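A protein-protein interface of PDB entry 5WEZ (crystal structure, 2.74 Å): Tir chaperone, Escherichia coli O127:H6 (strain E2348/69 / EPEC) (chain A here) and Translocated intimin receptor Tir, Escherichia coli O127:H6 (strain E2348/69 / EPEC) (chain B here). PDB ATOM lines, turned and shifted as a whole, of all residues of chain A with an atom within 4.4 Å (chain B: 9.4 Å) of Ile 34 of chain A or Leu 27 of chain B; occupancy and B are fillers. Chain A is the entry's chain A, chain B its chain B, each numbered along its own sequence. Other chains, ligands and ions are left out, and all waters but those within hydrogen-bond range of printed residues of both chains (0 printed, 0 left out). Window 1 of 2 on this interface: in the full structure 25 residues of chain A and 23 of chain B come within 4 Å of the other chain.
Of the 17 printed residues of chain B, 12 touch a printed residue of chain A.
Hydrophobic or aromatic side chains of chain B that line the printed part of chain A: Ile 21, Leu 27, Phe 33 and Pro 35.
Hydrophobic or aromatic side chains of chain A within 4 Å of the printed part of chain B: Phe 13, Ile 17, Phe 32, Ala 33 and Ile 34.
Among the printed residues, 21 pairs touch across the chains.
O of Ser 31 of chain B sits at hydrogen-bond distance from N of Asp 35 of chain A, 2.9 Å away.
The backbone carbonyl oxygen (O) of Ile 17 of chain A is in hydrogen-bond range of the backbone NH (N) of Ser 22 of chain B (3.1 Å).
The side-chain hydroxyl (OG) of Ser 29 of chain B sits at hydrogen-bond distance from the side-chain carboxylate (OD2) of Asp 35 of chain A (3.0 Å).
OE2 of Glu 111 of chain A sits at hydrogen-bond distance from N of Leu 27 of chain B (3.1 Å).
The side-chain carboxylate (OE2) of Glu 111 of chain A sits at hydrogen-bond distance from the backbone NH (N) of Ala 26 of chain B (3.2 Å).
OE2 of Glu 111 of chain A is in hydrogen-bond range of OG of Ser 23 of chain B.
The backbone carbonyl oxygen of Ala 33 of chain A is in hydrogen-bond range of the backbone NH of Phe 33 of chain B.
Among the printed residues, pairs that only touch across the chains: Ile 17 of chain A with Ile 21 of chain B, Glu 111 of chain A with Gly 25 of chain B, Phe 32 of chain A with Pro 35 of chain B, Phe 32 of chain A with Phe 33 of chain B, Glu 115 of chain A with Ala 26 of chain B, Glu 115 of chain A with Leu 27 of chain B, Ile 34 of chain A with Leu 27 of chain B, Ala 33 of chain A with Leu 32 of chain B, Ile 17 of chain A with Ser 23 of chain B, Asp 35 of chain A with Arg 30 of chain B, Ile 34 of chain A with Ser 31 of chain B, Ile 34 of chain A with Ser 29 of chain B, Ile 17 of chain A with Leu 27 of chain B and Phe 13 of chain A with Leu 27 of chain B.
O of His 19 of chain B lies within hydrogen-bond range of N of Leu 32 of chain B, 2.8 Å away.
The side-chain hydroxyl of Ser 23 of chain B sits at hydrogen-bond distance from the backbone NH of Gly 25 of chain B.
Ile 34 of chain A touches just these residues of chain B: Leu 27, Ser 29 and Ser 31.
Leu 27 of chain B touches five residues of chain A.
Of the printed residues of chain B, Asp 35 of chain A touches Ser 29, Arg 30 and Ser 31.
Printed residues of chain A within 4 Å of Ala 26 of chain B: Glu 111 (3.2 Å) and Glu 115 (3.3 Å).
Of the printed residues of chain A, Gly 25 of chain B touches Glu 111.
Of the printed residues of chain A, Ser 23 of chain B touches Ile 17 and Glu 111.
Thr 24 of chain B touches none of the printed residues of chain A.
Tyr 38 of chain A touches none of the printed residues of chain B.
The nearest printed residue of chain A that does not touch Phe 33 of chain B is Ile 34 of chain A (4.7 Å).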
ATOM      1  N   PHE A  13      -4.745 -13.680  -1.157  1.00  0.00           N
ATOM      2  CA  PHE A  13      -5.682 -12.570  -1.337  1.00  0.00           C
ATOM      3  C   PHE A  13      -5.300 -11.369  -0.471  1.00  0.00           C
ATOM      4  O   PHE A  13      -5.249 -10.226  -0.950  1.00  0.00           O
ATOM      5  CB  PHE A  13      -7.102 -13.073  -1.025  1.00  0.00           C
ATOM      6  CG  PHE A  13      -8.106 -12.013  -0.733  1.00  0.00           C
ATOM      7  CD1 PHE A  13      -8.933 -11.529  -1.738  1.00  0.00           C
ATOM      8  CD2 PHE A  13      -8.297 -11.551   0.564  1.00  0.00           C
ATOM      9  CE1 PHE A  13      -9.902 -10.573  -1.460  1.00  0.00           C
ATOM     10  CE2 PHE A  13      -9.261 -10.583   0.849  1.00  0.00           C
ATOM     11  CZ  PHE A  13     -10.066 -10.091  -0.162  1.00  0.00           C
ATOM     12  N   ILE A  17      -4.536  -7.344  -1.772  1.00  0.00           N
ATOM     13  CA  ILE A  17      -5.098  -6.046  -1.381  1.00  0.00           C
ATOM     14  C   ILE A  17      -4.233  -5.299  -0.373  1.00  0.00           C
ATOM     15  O   ILE A  17      -4.506  -4.121  -0.095  1.00  0.00           O
ATOM     16  CB  ILE A  17      -6.536  -6.134  -0.816  1.00  0.00           C
ATOM     17  CG1 ILE A  17      -6.675  -7.195   0.282  1.00  0.00           C
ATOM     18  CG2 ILE A  17      -7.555  -6.355  -1.925  1.00  0.00           C
ATOM     19  CD1 ILE A  17      -8.080  -7.247   0.852  1.00  0.00           C
ATOM     20  N   PHE A  32     -14.323 -10.240   8.201  1.00  0.00           N
ATOM     21  CA  PHE A  32     -13.759  -8.912   8.110  1.00  0.00           C
ATOM     22  C   PHE A  32     -14.884  -7.986   7.659  1.00  0.00           C
ATOM     23  O   PHE A  32     -15.795  -8.414   6.949  1.00  0.00           O
ATOM     24  CB  PHE A  32     -12.586  -8.884   7.125  1.00  0.00           C
ATOM     25  CG  PHE A  32     -12.968  -9.290   5.755  1.00  0.00           C
ATOM     26  CD1 PHE A  32     -13.517  -8.362   4.874  1.00  0.00           C
ATOM     27  CD2 PHE A  32     -12.819 -10.590   5.346  1.00  0.00           C
ATOM     28  CE1 PHE A  32     -13.911  -8.721   3.606  1.00  0.00           C
ATOM     29  CE2 PHE A  32     -13.200 -10.959   4.084  1.00  0.00           C
ATOM     30  CZ  PHE A  32     -13.755 -10.016   3.206  1.00  0.00           C
ATOM     31  N   ALA A  33     -14.845  -6.730   8.089  1.00  0.00           N
ATOM     32  CA  ALA A  33     -15.858  -5.762   7.701  1.00  0.00           C
ATOM     33  C   ALA A  33     -15.250  -4.735   6.754  1.00  0.00           C
ATOM     34  O   ALA A  33     -14.351  -3.977   7.134  1.00  0.00           O
ATOM     35  CB  ALA A  33     -16.466  -5.074   8.925  1.00  0.00           C
ATOM     36  N   ILE A  34     -15.741  -4.710   5.521  1.00  0.00           N
ATOM     37  CA  ILE A  34     -15.232  -3.775   4.527  1.00  0.00           C
ATOM     38  C   ILE A  34     -15.951  -2.445   4.725  1.00  0.00           C
ATOM     39  O   ILE A  34     -17.153  -2.325   4.466  1.00  0.00           O
ATOM     40  CB  ILE A  34     -15.393  -4.313   3.102  1.00  0.00           C
ATOM     41  CG1 ILE A  34     -14.242  -5.266   2.812  1.00  0.00           C
ATOM     42  CG2 ILE A  34     -15.387  -3.188   2.096  1.00  0.00           C
ATOM     43  CD1 ILE A  34     -13.938  -5.385   1.363  1.00  0.00           C
ATOM     44  N   ASP A  35     -15.206  -1.458   5.238  1.00  0.00           N
ATOM     45  CA  ASP A  35     -15.680  -0.104   5.508  1.00  0.00           C
ATOM     46  C   ASP A  35     -16.635  -0.039   6.697  1.00  0.00           C
ATOM     47  O   ASP A  35     -17.526   0.813   6.729  1.00  0.00           O
ATOM     48  CB  ASP A  35     -16.327   0.511   4.268  1.00  0.00           C
ATOM     49  CG  ASP A  35     -15.311   0.893   3.216  1.00  0.00           C
ATOM     50  OD1 ASP A  35     -14.096   0.644   3.418  1.00  0.00           O
ATOM     51  OD2 ASP A  35     -15.732   1.445   2.174  1.00  0.00           O
ATOM     52  N   GLU A  36     -16.455  -0.933   7.678  1.00  0.00           N
ATOM     53  CA  GLU A  36     -17.161  -0.926   8.964  1.00  0.00           C
ATOM     54  C   GLU A  36     -18.684  -0.836   8.848  1.00  0.00           C
ATOM     55  O   GLU A  36     -19.383  -0.682   9.858  1.00  0.00           O
ATOM     56  CB  GLU A  36     -16.621   0.207   9.857  1.00  0.00           C
ATOM     57  CG  GLU A  36     -17.266   1.583   9.701  1.00  0.00           C
ATOM     58  CD  GLU A  36     -16.407   2.694  10.276  1.00  0.00           C
ATOM     59  OE1 GLU A  36     -15.688   3.351   9.496  1.00  0.00           O
ATOM     60  OE2 GLU A  36     -16.435   2.901  11.506  1.00  0.00           O
ATOM     61  N   ILE A  37     -19.222  -0.948   7.639  1.00  0.00           N
ATOM     62  CA  ILE A  37     -20.661  -1.078   7.420  1.00  0.00           C
ATOM     63  C   ILE A  37     -20.997  -2.447   6.840  1.00  0.00           C
ATOM     64  O   ILE A  37     -21.890  -3.142   7.328  1.00  0.00           O
ATOM     65  CB  ILE A  37     -21.184   0.065   6.516  1.00  0.00           C
ATOM     66  CG1 ILE A  37     -20.550   1.384   6.923  1.00  0.00           C
ATOM     67  CG2 ILE A  37     -22.686   0.197   6.616  1.00  0.00           C
ATOM     68  CD1 ILE A  37     -21.284   2.623   6.437  1.00  0.00           C
ATOM     69  N   TYR A  38     -20.252  -2.870   5.827  1.00  0.00           N
ATOM     70  CA  TYR A  38     -20.542  -4.107   5.114  1.00  0.00           C
ATOM     71  C   TYR A  38     -19.777  -5.266   5.749  1.00  0.00           C
ATOM     72  O   TYR A  38     -18.576  -5.439   5.530  1.00  0.00           O
ATOM     73  CB  TYR A  38     -20.216  -3.937   3.637  1.00  0.00           C
ATOM     74  CG  TYR A  38     -20.841  -2.687   3.110  1.00  0.00           C
ATOM     75  CD1 TYR A  38     -22.215  -2.502   3.177  1.00  0.00           C
ATOM     76  CD2 TYR A  38     -20.063  -1.680   2.568  1.00  0.00           C
ATOM     77  CE1 TYR A  38     -22.802  -1.335   2.709  1.00  0.00           C
ATOM     78  CE2 TYR A  38     -20.640  -0.507   2.093  1.00  0.00           C
ATOM     79  CZ  TYR A  38     -22.006  -0.345   2.172  1.00  0.00           C
ATOM     80  OH  TYR A  38     -22.555   0.791   1.702  1.00  0.00           O
ATOM     81  N   GLU A 111     -11.239 -11.837  -4.561  1.00  0.00           N
ATOM     82  CA  GLU A 111     -11.473 -10.401  -4.466  1.00  0.00           C
ATOM     83  C   GLU A 111     -12.696  -9.970  -5.269  1.00  0.00           C
ATOM     84  O   GLU A 111     -13.523  -9.201  -4.775  1.00  0.00           O
ATOM     85  CB  GLU A 111     -10.217  -9.658  -4.918  1.00  0.00           C
ATOM     86  CG  GLU A 111     -10.415  -8.253  -5.353  1.00  0.00           C
ATOM     87  CD  GLU A 111      -9.203  -7.408  -5.077  1.00  0.00           C
ATOM     88  OE1 GLU A 111      -8.041  -7.882  -5.218  1.00  0.00           O
ATOM     89  OE2 GLU A 111      -9.432  -6.242  -4.707  1.00  0.00           O
ATOM     90  N   GLU A 115     -16.357  -8.372  -3.244  1.00  0.00           N
ATOM     91  CA  GLU A 115     -17.034  -7.109  -3.498  1.00  0.00           C
ATOM     92  C   GLU A 115     -18.373  -7.304  -4.203  1.00  0.00           C
ATOM     93  O   GLU A 115     -19.230  -6.416  -4.112  1.00  0.00           O
ATOM     94  CB  GLU A 115     -16.148  -6.146  -4.291  1.00  0.00           C
ATOM     95  CG  GLU A 115     -16.266  -4.630  -3.839  1.00  0.00           C
ATOM     96  CD  GLU A 115     -17.053  -3.772  -4.802  1.00  0.00           C
ATOM     97  OE1 GLU A 115     -17.328  -4.279  -5.904  1.00  0.00           O
ATOM     98  OE2 GLU A 115     -17.397  -2.592  -4.473  1.00  0.00           O
ATOM     99  N   HIS B  19      -7.351  -1.211   7.869  1.00  0.00           N
ATOM    100  CA  HIS B  19      -6.312  -1.594   6.943  1.00  0.00           C
ATOM    101  C   HIS B  19      -6.713  -0.973   5.611  1.00  0.00           C
ATOM    102  O   HIS B  19      -7.888  -1.031   5.176  1.00  0.00           O
ATOM    103  CB  HIS B  19      -6.144  -3.100   6.864  1.00  0.00           C
ATOM    104  CG  HIS B  19      -5.180  -3.639   7.869  1.00  0.00           C
ATOM    105  ND1 HIS B  19      -4.344  -4.700   7.606  1.00  0.00           N
ATOM    106  CD2 HIS B  19      -4.919  -3.258   9.140  1.00  0.00           C
ATOM    107  CE1 HIS B  19      -3.613  -4.953   8.676  1.00  0.00           C
ATOM    108  NE2 HIS B  19      -3.941  -4.091   9.619  1.00  0.00           N
ATOM    109  N   LEU B  20      -5.726  -0.352   4.986  1.00  0.00           N
ATOM    110  CA  LEU B  20      -5.908   0.315   3.720  1.00  0.00           C
ATOM    111  C   LEU B  20      -5.392  -0.593   2.626  1.00  0.00           C
ATOM    112  O   LEU B  20      -4.275  -1.136   2.734  1.00  0.00           O
ATOM    113  CB  LEU B  20      -5.160   1.640   3.711  1.00  0.00           C
ATOM    114  N   ILE B  21      -6.235  -0.720   1.597  1.00  0.00           N
ATOM    115  CA  ILE B  21      -6.078  -1.546   0.405  1.00  0.00           C
ATOM    116  C   ILE B  21      -5.496  -0.776  -0.758  1.00  0.00           C
ATOM    117  O   ILE B  21      -6.031   0.233  -1.131  1.00  0.00           O
ATOM    118  CB  ILE B  21      -7.472  -1.920  -0.085  1.00  0.00           C
ATOM    119  CG1 ILE B  21      -8.307  -2.502   1.058  1.00  0.00           C
ATOM    120  CG2 ILE B  21      -7.387  -2.841  -1.292  1.00  0.00           C
ATOM    121  CD1 ILE B  21      -8.813  -1.483   2.054  1.00  0.00           C
ATOM    122  N   SER B  22      -4.429  -1.258  -1.366  1.00  0.00           N
ATOM    123  CA  SER B  22      -3.844  -0.546  -2.492  1.00  0.00           C
ATOM    124  C   SER B  22      -3.715  -1.555  -3.610  1.00  0.00           C
ATOM    125  O   SER B  22      -2.643  -1.812  -4.093  1.00  0.00           O
ATOM    126  CB  SER B  22      -2.491  -0.036  -2.067  1.00  0.00           C
ATOM    127  OG  SER B  22      -2.224  -0.504  -0.764  1.00  0.00           O
ATOM    128  N   SER B  23      -4.829  -2.116  -4.034  1.00  0.00           N
ATOM    129  CA  SER B  23      -4.839  -3.208  -4.992  1.00  0.00           C
ATOM    130  C   SER B  23      -5.477  -2.773  -6.299  1.00  0.00           C
ATOM    131  O   SER B  23      -6.311  -1.874  -6.329  1.00  0.00           O
ATOM    132  CB  SER B  23      -5.619  -4.393  -4.466  1.00  0.00           C
ATOM    133  OG  SER B  23      -6.986  -4.251  -4.815  1.00  0.00           O
ATOM    134  N   THR B  24      -5.068  -3.439  -7.386  1.00  0.00           N
ATOM    135  CA  THR B  24      -5.733  -3.323  -8.680  1.00  0.00           C
ATOM    136  C   THR B  24      -7.113  -3.948  -8.654  1.00  0.00           C
ATOM    137  O   THR B  24      -7.999  -3.502  -9.388  1.00  0.00           O
ATOM    138  CB  THR B  24      -4.897  -4.001  -9.775  1.00  0.00           C
ATOM    139  OG1 THR B  24      -3.714  -3.225 -10.041  1.00  0.00           O
ATOM    140  CG2 THR B  24      -5.697  -4.190 -11.074  1.00  0.00           C
ATOM    141  N   GLY B  25      -7.308  -4.949  -7.812  1.00  0.00           N
ATOM    142  CA  GLY B  25      -8.534  -5.707  -7.779  1.00  0.00           C
ATOM    143  C   GLY B  25      -9.810  -4.923  -7.510  1.00  0.00           C
ATOM    144  O   GLY B  25      -9.816  -3.718  -7.273  1.00  0.00           O
ATOM    145  N   ALA B  26     -10.918  -5.649  -7.529  1.00  0.00           N
ATOM    146  CA  ALA B  26     -12.237  -5.041  -7.526  1.00  0.00           C
ATOM    147  C   ALA B  26     -12.627  -4.458  -6.207  1.00  0.00           C
ATOM    148  O   ALA B  26     -13.819  -4.251  -6.006  1.00  0.00           O
ATOM    149  CB  ALA B  26     -13.300  -6.065  -7.927  1.00  0.00           C
ATOM    150  N   LEU B  27     -11.689  -4.212  -5.303  1.00  0.00           N
ATOM    151  CA  LEU B  27     -11.969  -3.561  -4.032  1.00  0.00           C
ATOM    152  C   LEU B  27     -11.393  -2.136  -4.031  1.00  0.00           C
ATOM    153  O   LEU B  27     -10.452  -1.820  -3.298  1.00  0.00           O
ATOM    154  CB  LEU B  27     -11.421  -4.427  -2.841  1.00  0.00           C
ATOM    155  CG  LEU B  27     -12.161  -5.743  -2.565  1.00  0.00           C
ATOM    156  CD1 LEU B  27     -11.483  -6.633  -1.516  1.00  0.00           C
ATOM    157  CD2 LEU B  27     -13.556  -5.474  -2.104  1.00  0.00           C
ATOM    158  N   GLY B  28     -11.979  -1.270  -4.867  1.00  0.00           N
ATOM    159  CA  GLY B  28     -11.623   0.141  -4.952  1.00  0.00           C
ATOM    160  C   GLY B  28     -12.258   0.917  -3.819  1.00  0.00           C
ATOM    161  O   GLY B  28     -13.056   1.838  -4.036  1.00  0.00           O
ATOM    162  N   SER B  29     -11.888   0.545  -2.600  1.00  0.00           N
ATOM    163  CA  SER B  29     -12.599   0.948  -1.403  1.00  0.00           C
ATOM    164  C   SER B  29     -11.570   1.157  -0.307  1.00  0.00           C
ATOM    165  O   SER B  29     -10.454   0.649  -0.388  1.00  0.00           O
ATOM    166  CB  SER B  29     -13.647  -0.102  -1.008  1.00  0.00           C
ATOM    167  OG  SER B  29     -13.858  -0.078   0.388  1.00  0.00           O
ATOM    168  N   ARG B  30     -11.947   1.908   0.725  1.00  0.00           N
ATOM    169  CA  ARG B  30     -10.921   2.536   1.549  1.00  0.00           C
ATOM    170  C   ARG B  30     -10.300   1.583   2.573  1.00  0.00           C
ATOM    171  O   ARG B  30      -9.072   1.428   2.613  1.00  0.00           O
ATOM    172  CB  ARG B  30     -11.496   3.775   2.242  1.00  0.00           C
ATOM    173  N   SER B  31     -11.084   1.019   3.477  1.00  0.00           N
ATOM    174  CA  SER B  31     -10.467   0.190   4.506  1.00  0.00           C
ATOM    175  C   SER B  31     -11.236  -1.053   4.883  1.00  0.00           C
ATOM    176  O   SER B  31     -12.424  -1.104   4.669  1.00  0.00           O
ATOM    177  CB  SER B  31     -10.220   1.030   5.753  1.00  0.00           C
ATOM    178  OG  SER B  31     -11.328   0.997   6.636  1.00  0.00           O
ATOM    179  N   LEU B  32     -10.524  -1.990   5.502  1.00  0.00           N
ATOM    180  CA  LEU B  32     -11.087  -3.230   5.991  1.00  0.00           C
ATOM    181  C   LEU B  32     -10.893  -3.306   7.493  1.00  0.00           C
ATOM    182  O   LEU B  32      -9.780  -3.142   7.984  1.00  0.00           O
ATOM    183  CB  LEU B  32     -10.410  -4.419   5.317  1.00  0.00           C
ATOM    184  CG  LEU B  32      -9.174  -5.064   5.937  1.00  0.00           C
ATOM    185  CD1 LEU B  32      -9.496  -5.772   7.240  1.00  0.00           C
ATOM    186  CD2 LEU B  32      -8.596  -6.058   4.948  1.00  0.00           C
ATOM    187  N   PHE B  33     -11.957  -3.612   8.205  1.00  0.00           N
ATOM    188  CA  PHE B  33     -11.880  -3.753   9.635  1.00  0.00           C
ATOM    189  C   PHE B  33     -12.194  -5.203   9.890  1.00  0.00           C
ATOM    190  O   PHE B  33     -13.061  -5.778   9.243  1.00  0.00           O
ATOM    191  CB  PHE B  33     -12.882  -2.847  10.330  1.00  0.00           C
ATOM    192  N   SER B  34     -11.471  -5.792  10.821  1.00  0.00           N
ATOM    193  CA  SER B  34     -11.650  -7.185  11.150  1.00  0.00           C
ATOM    194  C   SER B  34     -12.404  -7.351  12.449  1.00  0.00           C
ATOM    195  O   SER B  34     -12.035  -6.781  13.476  1.00  0.00           O
ATOM    196  CB  SER B  34     -10.287  -7.821  11.254  1.00  0.00           C
ATOM    197  OG  SER B  34      -9.346  -6.978  10.620  1.00  0.00           O
ATOM    198  N   PRO B  35     -13.511  -8.184  12.371  1.00  0.00           N
ATOM    199  CA  PRO B  35     -14.260  -8.344  13.614  1.00  0.00           C
ATOM    200  C   PRO B  35     -13.889  -9.656  14.266  1.00  0.00           C
ATOM    201  O   PRO B  35     -13.980 -10.722  13.663  1.00  0.00           O
ATOM    202  CB  PRO B  35     -15.711  -8.398  13.140  1.00  0.00           C
ATOM    203  CG  PRO B  35     -15.667  -8.788  11.699  1.00  0.00           C
ATOM    204  CD  PRO B  35     -14.242  -9.029  11.337  1.00  0.00           C
